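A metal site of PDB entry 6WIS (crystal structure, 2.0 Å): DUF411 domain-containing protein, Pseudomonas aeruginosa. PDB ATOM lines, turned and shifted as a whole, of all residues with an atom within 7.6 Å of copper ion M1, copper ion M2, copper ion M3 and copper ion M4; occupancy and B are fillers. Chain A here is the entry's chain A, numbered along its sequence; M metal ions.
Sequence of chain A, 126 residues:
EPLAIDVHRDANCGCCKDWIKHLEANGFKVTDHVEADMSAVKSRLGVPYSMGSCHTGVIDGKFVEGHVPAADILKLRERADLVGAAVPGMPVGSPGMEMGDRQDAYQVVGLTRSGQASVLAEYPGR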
ATOM      1  N   VAL A   7      33.655 -22.273  14.421  1.00  0.00           N
ATOM      2  CA  VAL A   7      32.947 -21.492  15.442  1.00  0.00           C
ATOM      3  C   VAL A   7      33.896 -21.118  16.564  1.00  0.00           C
ATOM      4  O   VAL A   7      34.546 -21.987  17.174  1.00  0.00           O
ATOM      5  CB  VAL A   7      31.731 -22.260  15.975  1.00  0.00           C
ATOM      6  CG1 VAL A   7      30.998 -21.412  17.044  1.00  0.00           C
ATOM      7  CG2 VAL A   7      30.779 -22.602  14.809  1.00  0.00           C
ATOM      8  N   HIS A   8      33.976 -19.816  16.853  1.00  0.00           N
ATOM      9  CA  HIS A   8      34.647 -19.289  18.037  1.00  0.00           C
ATOM     10  C   HIS A   8      33.556 -18.932  19.039  1.00  0.00           C
ATOM     11  O   HIS A   8      32.689 -18.102  18.730  1.00  0.00           O
ATOM     12  CB  HIS A   8      35.484 -18.039  17.716  1.00  0.00           C
ATOM     13  CG  HIS A   8      36.207 -18.111  16.413  1.00  0.00           C
ATOM     14  ND1 HIS A   8      37.581 -18.246  16.324  1.00  0.00           N
ATOM     15  CD2 HIS A   8      35.759 -18.048  15.137  1.00  0.00           C
ATOM     16  CE1 HIS A   8      37.940 -18.274  15.063  1.00  0.00           C
ATOM     17  NE2 HIS A   8      36.854 -18.157  14.317  1.00  0.00           N
ATOM     18  N   ARG A   9      33.575 -19.565  20.214  1.00  0.00           N
ATOM     19  CA  ARG A   9      32.442 -19.407  21.137  1.00  0.00           C
ATOM     20  C   ARG A   9      32.894 -18.999  22.526  1.00  0.00           C
ATOM     21  O   ARG A   9      33.992 -19.323  22.982  1.00  0.00           O
ATOM     22  CB  ARG A   9      31.611 -20.700  21.206  1.00  0.00           C
ATOM     23  CG  ARG A   9      32.377 -21.937  21.655  1.00  0.00           C
ATOM     24  CD  ARG A   9      31.444 -23.134  21.844  1.00  0.00           C
ATOM     25  NE  ARG A   9      32.161 -24.397  21.978  1.00  0.00           N
ATOM     26  CZ  ARG A   9      32.436 -25.003  23.131  1.00  0.00           C
ATOM     27  NH1 ARG A   9      32.062 -24.480  24.294  1.00  0.00           N
ATOM     28  NH2 ARG A   9      33.079 -26.169  23.126  1.00  0.00           N
ATOM     29  N   ASP A  10      32.001 -18.277  23.204  1.00  0.00           N
ATOM     30  CA  ASP A  10      32.204 -17.847  24.590  1.00  0.00           C
ATOM     31  C   ASP A  10      32.449 -19.039  25.501  1.00  0.00           C
ATOM     32  O   ASP A  10      31.872 -20.118  25.321  1.00  0.00           O
ATOM     33  CB  ASP A  10      30.989 -17.074  25.080  1.00  0.00           C
ATOM     34  CG  ASP A  10      31.035 -15.625  24.692  1.00  0.00           C
ATOM     35  OD1 ASP A  10      32.040 -15.197  24.076  1.00  0.00           O
ATOM     36  OD2 ASP A  10      30.078 -14.892  25.014  1.00  0.00           O
ATOM     37  N   ALA A  11      33.329 -18.856  26.477  1.00  0.00           N
ATOM     38  CA  ALA A  11      33.520 -19.906  27.476  1.00  0.00           C
ATOM     39  C   ALA A  11      32.253 -20.094  28.285  1.00  0.00           C
ATOM     40  O   ALA A  11      31.523 -19.126  28.563  1.00  0.00           O
ATOM     41  CB  ALA A  11      34.698 -19.564  28.404  1.00  0.00           C
ATOM     42  N   ASN A  12      31.962 -21.353  28.655  1.00  0.00           N
ATOM     43  CA  ASN A  12      30.908 -21.703  29.627  1.00  0.00           C
ATOM     44  C   ASN A  12      29.522 -21.264  29.145  1.00  0.00           C
ATOM     45  O   ASN A  12      28.692 -20.812  29.927  1.00  0.00           O
ATOM     46  CB  ASN A  12      31.204 -21.115  31.016  1.00  0.00           C
ATOM     47  CG  ASN A  12      30.276 -21.703  32.089  1.00  0.00           C
ATOM     48  OD1 ASN A  12      30.144 -22.929  32.198  1.00  0.00           O
ATOM     49  ND2 ASN A  12      29.600 -20.841  32.844  1.00  0.00           N
ATOM     50  N   CYS A  13      29.276 -21.391  27.843  1.00  0.00           N
ATOM     51  CA  CYS A  13      28.037 -20.936  27.226  1.00  0.00           C
ATOM     52  C   CYS A  13      27.369 -22.163  26.606  1.00  0.00           C
ATOM     53  O   CYS A  13      27.887 -22.725  25.627  1.00  0.00           O
ATOM     54  CB  CYS A  13      28.316 -19.843  26.192  1.00  0.00           C
ATOM     55  SG  CYS A  13      26.869 -18.922  25.630  1.00  0.00           S
ATOM     56  N   GLY A  14      26.254 -22.589  27.187  1.00  0.00           N
ATOM     57  CA  GLY A  14      25.591 -23.812  26.779  1.00  0.00           C
ATOM     58  C   GLY A  14      24.848 -23.673  25.461  1.00  0.00           C
ATOM     59  O   GLY A  14      24.843 -24.616  24.665  1.00  0.00           O
ATOM     60  N   CYS A  15      24.262 -22.491  25.222  1.00  0.00           N
ATOM     61  CA  CYS A  15      23.493 -22.263  23.993  1.00  0.00           C
ATOM     62  C   CYS A  15      24.363 -22.362  22.740  1.00  0.00           C
ATOM     63  O   CYS A  15      23.897 -22.855  21.705  1.00  0.00           O
ATOM     64  CB  CYS A  15      22.797 -20.900  24.051  1.00  0.00           C
ATOM     65  SG  CYS A  15      23.962 -19.629  24.601  1.00  0.00           S
ATOM     66  N   CYS A  16      25.618 -21.897  22.804  1.00  0.00           N
ATOM     67  CA  CYS A  16      26.521 -22.046  21.652  1.00  0.00           C
ATOM     68  C   CYS A  16      26.675 -23.501  21.248  1.00  0.00           C
ATOM     69  O   CYS A  16      26.661 -23.825  20.058  1.00  0.00           O
ATOM     70  CB  CYS A  16      27.907 -21.459  21.949  1.00  0.00           C
ATOM     71  SG  CYS A  16      27.989 -19.797  22.696  1.00  0.00           S
ATOM     72  N   LYS A  17      26.851 -24.391  22.226  1.00  0.00           N
ATOM     73  CA  LYS A  17      27.001 -25.813  21.942  1.00  0.00           C
ATOM     74  C   LYS A  17      25.720 -26.417  21.386  1.00  0.00           C
ATOM     75  O   LYS A  17      25.784 -27.315  20.535  1.00  0.00           O
ATOM     76  CB  LYS A  17      27.416 -26.562  23.228  1.00  0.00           C
ATOM     77  CG  LYS A  17      28.844 -26.232  23.722  1.00  0.00           C
ATOM     78  CD  LYS A  17      29.124 -26.824  25.118  1.00  0.00           C
ATOM     79  N   ASP A  18      24.565 -25.937  21.850  1.00  0.00           N
ATOM     80  CA  ASP A  18      23.284 -26.396  21.313  1.00  0.00           C
ATOM     81  C   ASP A  18      23.113 -25.929  19.871  1.00  0.00           C
ATOM     82  O   ASP A  18      22.678 -26.694  19.005  1.00  0.00           O
ATOM     83  CB  ASP A  18      22.146 -25.873  22.207  1.00  0.00           C
ATOM     84  CG  ASP A  18      20.765 -26.469  21.859  1.00  0.00           C
ATOM     85  OD1 ASP A  18      20.658 -27.529  21.230  1.00  0.00           O
ATOM     86  OD2 ASP A  18      19.753 -25.875  22.241  1.00  0.00           O
ATOM     87  N   TRP A  19      23.462 -24.663  19.583  1.00  0.00           N
ATOM     88  CA  TRP A  19      23.419 -24.178  18.201  1.00  0.00           C
ATOM     89  C   TRP A  19      24.315 -25.021  17.288  1.00  0.00           C
ATOM     90  O   TRP A  19      23.910 -25.372  16.171  1.00  0.00           O
ATOM     91  CB  TRP A  19      23.834 -22.712  18.181  1.00  0.00           C
ATOM     92  CG  TRP A  19      23.845 -22.054  16.878  1.00  0.00           C
ATOM     93  CD1 TRP A  19      22.757 -21.647  16.160  1.00  0.00           C
ATOM     94  CD2 TRP A  19      24.995 -21.655  16.120  1.00  0.00           C
ATOM     95  NE1 TRP A  19      23.168 -21.013  14.990  1.00  0.00           N
ATOM     96  CE2 TRP A  19      24.544 -20.991  14.959  1.00  0.00           C
ATOM     97  CE3 TRP A  19      26.379 -21.783  16.334  1.00  0.00           C
ATOM     98  CZ2 TRP A  19      25.422 -20.460  14.009  1.00  0.00           C
ATOM     99  CZ3 TRP A  19      27.260 -21.239  15.373  1.00  0.00           C
ATOM    100  CH2 TRP A  19      26.780 -20.601  14.228  1.00  0.00           C
ATOM    101  N   MET A  38      37.990 -12.706  22.046  1.00  0.00           N
ATOM    102  CA  MET A  38      36.788 -12.580  21.247  1.00  0.00           C
ATOM    103  C   MET A  38      36.665 -11.182  20.615  1.00  0.00           C
ATOM    104  O   MET A  38      36.160 -11.057  19.495  1.00  0.00           O
ATOM    105  CB  MET A  38      35.546 -12.901  22.083  1.00  0.00           C
ATOM    106  CG  MET A  38      34.270 -12.867  21.251  1.00  0.00           C
ATOM    107  SD  MET A  38      34.253 -14.354  19.943  1.00  0.00           S
ATOM    108  CE  MET A  38      33.457 -15.680  21.096  1.00  0.00           C
ATOM    109  N   SER A  53      27.292 -11.140  19.679  1.00  0.00           N
ATOM    110  CA  SER A  53      26.508 -12.183  20.331  1.00  0.00           C
ATOM    111  C   SER A  53      27.500 -13.016  21.108  1.00  0.00           C
ATOM    112  O   SER A  53      28.619 -12.573  21.408  1.00  0.00           O
ATOM    113  CB  SER A  53      25.687 -12.951  19.281  1.00  0.00           C
ATOM    114  OG  SER A  53      24.786 -13.875  19.869  1.00  0.00           O
ATOM    115  N   CYS A  54      27.113 -14.256  21.440  1.00  0.00           N
ATOM    116  CA  CYS A  54      27.899 -15.146  22.294  1.00  0.00           C
ATOM    117  C   CYS A  54      28.876 -16.027  21.524  1.00  0.00           C
ATOM    118  O   CYS A  54      29.719 -16.712  22.140  1.00  0.00           O
ATOM    119  CB  CYS A  54      26.930 -16.035  23.083  1.00  0.00           C
ATOM    120  SG  CYS A  54      25.650 -16.729  21.956  1.00  0.00           S
ATOM    121  N   HIS A  55      28.781 -16.080  20.194  1.00  0.00           N
ATOM    122  CA  HIS A  55      29.721 -16.868  19.412  1.00  0.00           C
ATOM    123  C   HIS A  55      29.830 -16.262  18.017  1.00  0.00           C
ATOM    124  O   HIS A  55      28.948 -15.518  17.585  1.00  0.00           O
ATOM    125  CB  HIS A  55      29.289 -18.343  19.323  1.00  0.00           C
ATOM    126  CG  HIS A  55      27.996 -18.540  18.574  1.00  0.00           C
ATOM    127  ND1 HIS A  55      26.811 -18.879  19.190  1.00  0.00           N
ATOM    128  CD2 HIS A  55      27.713 -18.441  17.250  1.00  0.00           C
ATOM    129  CE1 HIS A  55      25.847 -18.981  18.281  1.00  0.00           C
ATOM    130  NE2 HIS A  55      26.369 -18.694  17.091  1.00  0.00           N
ATOM    131  N   THR A  56      30.893 -16.609  17.302  1.00  0.00           N
ATOM    132  CA  THR A  56      31.117 -16.103  15.948  1.00  0.00           C
ATOM    133  C   THR A  56      31.550 -17.276  15.073  1.00  0.00           C
ATOM    134  O   THR A  56      32.560 -17.924  15.366  1.00  0.00           O
ATOM    135  CB  THR A  56      32.199 -15.009  15.907  1.00  0.00           C
ATOM    136  OG1 THR A  56      31.858 -13.958  16.829  1.00  0.00           O
ATOM    137  CG2 THR A  56      32.295 -14.432  14.486  1.00  0.00           C
ATOM    138  N   GLU A  65      27.183 -14.358  13.125  1.00  0.00           N
ATOM    139  CA  GLU A  65      27.244 -13.853  14.496  1.00  0.00           C
ATOM    140  C   GLU A  65      25.990 -14.303  15.232  1.00  0.00           C
ATOM    141  O   GLU A  65      24.872 -13.933  14.847  1.00  0.00           O
ATOM    142  CB  GLU A  65      27.366 -12.331  14.506  1.00  0.00           C
ATOM    143  CG  GLU A  65      27.523 -11.734  15.906  1.00  0.00           C
ATOM    144  CD  GLU A  65      28.871 -12.079  16.548  1.00  0.00           C
ATOM    145  OE1 GLU A  65      29.743 -12.577  15.805  1.00  0.00           O
ATOM    146  OE2 GLU A  65      29.057 -11.859  17.781  1.00  0.00           O
ATOM    147  N   GLY A  66      26.157 -15.109  16.256  1.00  0.00           N
ATOM    148  CA  GLY A  66      25.002 -15.488  17.043  1.00  0.00           C
ATOM    149  C   GLY A  66      24.163 -16.631  16.462  1.00  0.00           C
ATOM    150  O   GLY A  66      24.580 -17.422  15.599  1.00  0.00           O
ATOM    151  N   HIS A  67      22.949 -16.716  16.991  1.00  0.00           N
ATOM    152  CA  HIS A  67      22.076 -17.875  16.772  1.00  0.00           C
ATOM    153  C   HIS A  67      21.308 -17.759  15.440  1.00  0.00           C
ATOM    154  O   HIS A  67      20.079 -17.743  15.394  1.00  0.00           O
ATOM    155  CB  HIS A  67      21.158 -18.023  17.971  1.00  0.00           C
ATOM    156  CG  HIS A  67      21.877 -18.465  19.205  1.00  0.00           C
ATOM    157  ND1 HIS A  67      22.003 -19.796  19.557  1.00  0.00           N
ATOM    158  CD2 HIS A  67      22.579 -17.779  20.138  1.00  0.00           C
ATOM    159  CE1 HIS A  67      22.730 -19.900  20.651  1.00  0.00           C
ATOM    160  NE2 HIS A  67      23.098 -18.689  21.025  1.00  0.00           N
ATOM    161  N   GLY A  89      22.856 -10.354  20.289  1.00  0.00           N
ATOM    162  CA  GLY A  89      22.337 -10.795  21.571  1.00  0.00           C
ATOM    163  C   GLY A  89      22.037 -12.294  21.576  1.00  0.00           C
ATOM    164  O   GLY A  89      22.674 -13.097  20.883  1.00  0.00           O
ATOM    165  N   MET A  90      21.044 -12.670  22.388  1.00  0.00           N
ATOM    166  CA  MET A  90      20.637 -14.065  22.452  1.00  0.00           C
ATOM    167  C   MET A  90      19.141 -14.147  22.648  1.00  0.00           C
ATOM    168  O   MET A  90      18.685 -14.390  23.763  1.00  0.00           O
ATOM    169  CB  MET A  90      21.357 -14.797  23.598  1.00  0.00           C
ATOM    170  CG  MET A  90      22.880 -14.802  23.557  1.00  0.00           C
ATOM    171  SD  MET A  90      23.696 -15.764  25.082  1.00  0.00           S
ATOM    172  CE  MET A  90      22.956 -14.718  26.563  1.00  0.00           C
ATOM    173  N   PRO A  91      18.390 -13.943  21.570  1.00  0.00           N
ATOM    174  CA  PRO A  91      16.915 -13.959  21.687  1.00  0.00           C
ATOM    175  C   PRO A  91      16.415 -15.354  21.977  1.00  0.00           C
ATOM    176  O   PRO A  91      16.827 -16.325  21.333  1.00  0.00           O
ATOM    177  CB  PRO A  91      16.439 -13.464  20.319  1.00  0.00           C
ATOM    178  CG  PRO A  91      17.603 -13.706  19.398  1.00  0.00           C
ATOM    179  CD  PRO A  91      18.844 -13.557  20.221  1.00  0.00           C
ATOM    180  N   SER A  94      15.440 -18.560  19.341  1.00  0.00           N
ATOM    181  CA  SER A  94      16.329 -18.783  18.217  1.00  0.00           C
ATOM    182  C   SER A  94      17.017 -20.138  18.373  1.00  0.00           C
ATOM    183  O   SER A  94      17.054 -20.695  19.478  1.00  0.00           O
ATOM    184  CB  SER A  94      17.351 -17.642  18.110  1.00  0.00           C
ATOM    185  OG  SER A  94      18.229 -17.604  19.231  1.00  0.00           O
ATOM    186  N   PRO A  95      17.541 -20.709  17.283  1.00  0.00           N
ATOM    187  CA  PRO A  95      18.088 -22.079  17.370  1.00  0.00           C
ATOM    188  C   PRO A  95      19.273 -22.157  18.320  1.00  0.00           C
ATOM    189  O   PRO A  95      20.218 -21.377  18.234  1.00  0.00           O
ATOM    190  CB  PRO A  95      18.502 -22.404  15.932  1.00  0.00           C
ATOM    191  CG  PRO A  95      17.845 -21.372  15.057  1.00  0.00           C
ATOM    192  CD  PRO A  95      17.553 -20.174  15.908  1.00  0.00           C
ATOM    193  N   GLY A  96      19.217 -23.129  19.230  1.00  0.00           N
ATOM    194  CA  GLY A  96      20.197 -23.231  20.295  1.00  0.00           C
ATOM    195  C   GLY A  96      19.873 -22.415  21.517  1.00  0.00           C
ATOM    196  O   GLY A  96      20.506 -22.621  22.563  1.00  0.00           O
ATOM    197  N   MET A  97      18.889 -21.530  21.445  1.00  0.00           N
ATOM    198  CA  MET A  97      18.412 -20.701  22.558  1.00  0.00           C
ATOM    199  C   MET A  97      16.929 -21.010  22.821  1.00  0.00           C
ATOM    200  O   MET A  97      16.220 -20.232  23.426  1.00  0.00           O
ATOM    201  CB  MET A  97      18.590 -19.208  22.258  1.00  0.00           C
ATOM    202  CG  MET A  97      19.994 -18.567  22.670  1.00  0.00           C
ATOM    203  SD  MET A  97      20.350 -18.684  24.614  1.00  0.00           S
ATOM    204  CE  MET A  97      18.793 -17.577  25.130  1.00  0.00           C
ATOM    205  N   MET A  99      13.561 -22.280  24.406  1.00  0.00           N
ATOM    206  CA  MET A  99      13.121 -22.648  25.752  1.00  0.00           C
ATOM    207  C   MET A  99      11.581 -22.663  25.828  1.00  0.00           C
ATOM    208  O   MET A  99      10.982 -21.796  26.469  1.00  0.00           O
ATOM    209  CB  MET A  99      13.683 -21.662  26.784  1.00  0.00           C
ATOM    210  CG  MET A  99      15.205 -21.612  26.820  1.00  0.00           C
ATOM    211  SD  MET A  99      15.959 -20.396  28.087  1.00  0.00           S
ATOM    212  CE  MET A  99      17.779 -20.613  27.520  1.00  0.00           C
HETATM  213 CU    CU M   1      26.783 -18.593  21.353  1.00  0.00          CU
HETATM  214 CU    CU M   2      24.291 -18.392  22.736  1.00  0.00          CU
HETATM  215 CU    CU M   3      26.124 -20.158  23.895  1.00  0.00          CU
HETATM  216 CU    CU M   4      22.530 -17.880  25.239  1.00  0.00          CU
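The backbone carbonyl oxygen (O) of Cys 54 sits at hydrogen-bond distance from the backbone NH (N) of Asp 10, at 3.0 Å.
The side-chain hydroxyl (OG) of Ser 53 lies close to the side-chain sulfur (SG) of Cys 54, at 3.6 Å.
NE2 of His 55 sits at hydrogen-bond distance from O of Gly 66, at 2.7 Å.
ND1 of His 67 sits at hydrogen-bond distance from O of Pro 95.
Three residues have an atom within 4 Å of copper ion M4: Cys 15, Met 90 and Met 97.
Of the 29 residues printed, 6 come within 4 Å of copper ion M2.
The nearest printed residue that does not touch copper ion M2 is Met 97 (4.3 Å).
Copper ion M3 is bound by N of Cys 16, SG of Cys 16, SG of Cys 13 and SG of Cys 15.
Copper ion M3 has four donor atoms within binding distance.
The nearest printed residue that does not touch copper ion M3 is Gly 14 (4.1 Å).
Copper ion M1 is bound by SG of Cys 16 (2.2 Å).
Copper ion M1 is bound by ND1 of His 55, at 2.2 Å.
Copper ion M1 is bound by SG of Cys 54.
Copper ion M4 is bound by SG of Cys 15 (2.3 Å).
SD of Met 97 binds copper ion M4, 2.4 Å away.
Copper ion M4 is bound by SD of Met 90 (2.4 Å).
Copper ion M2 is bound by NE2 of His 67.
Copper ion M2 is bound by SG of Cys 15 (2.3 Å).
Copper ion M2 is bound by SG of Cys 54.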
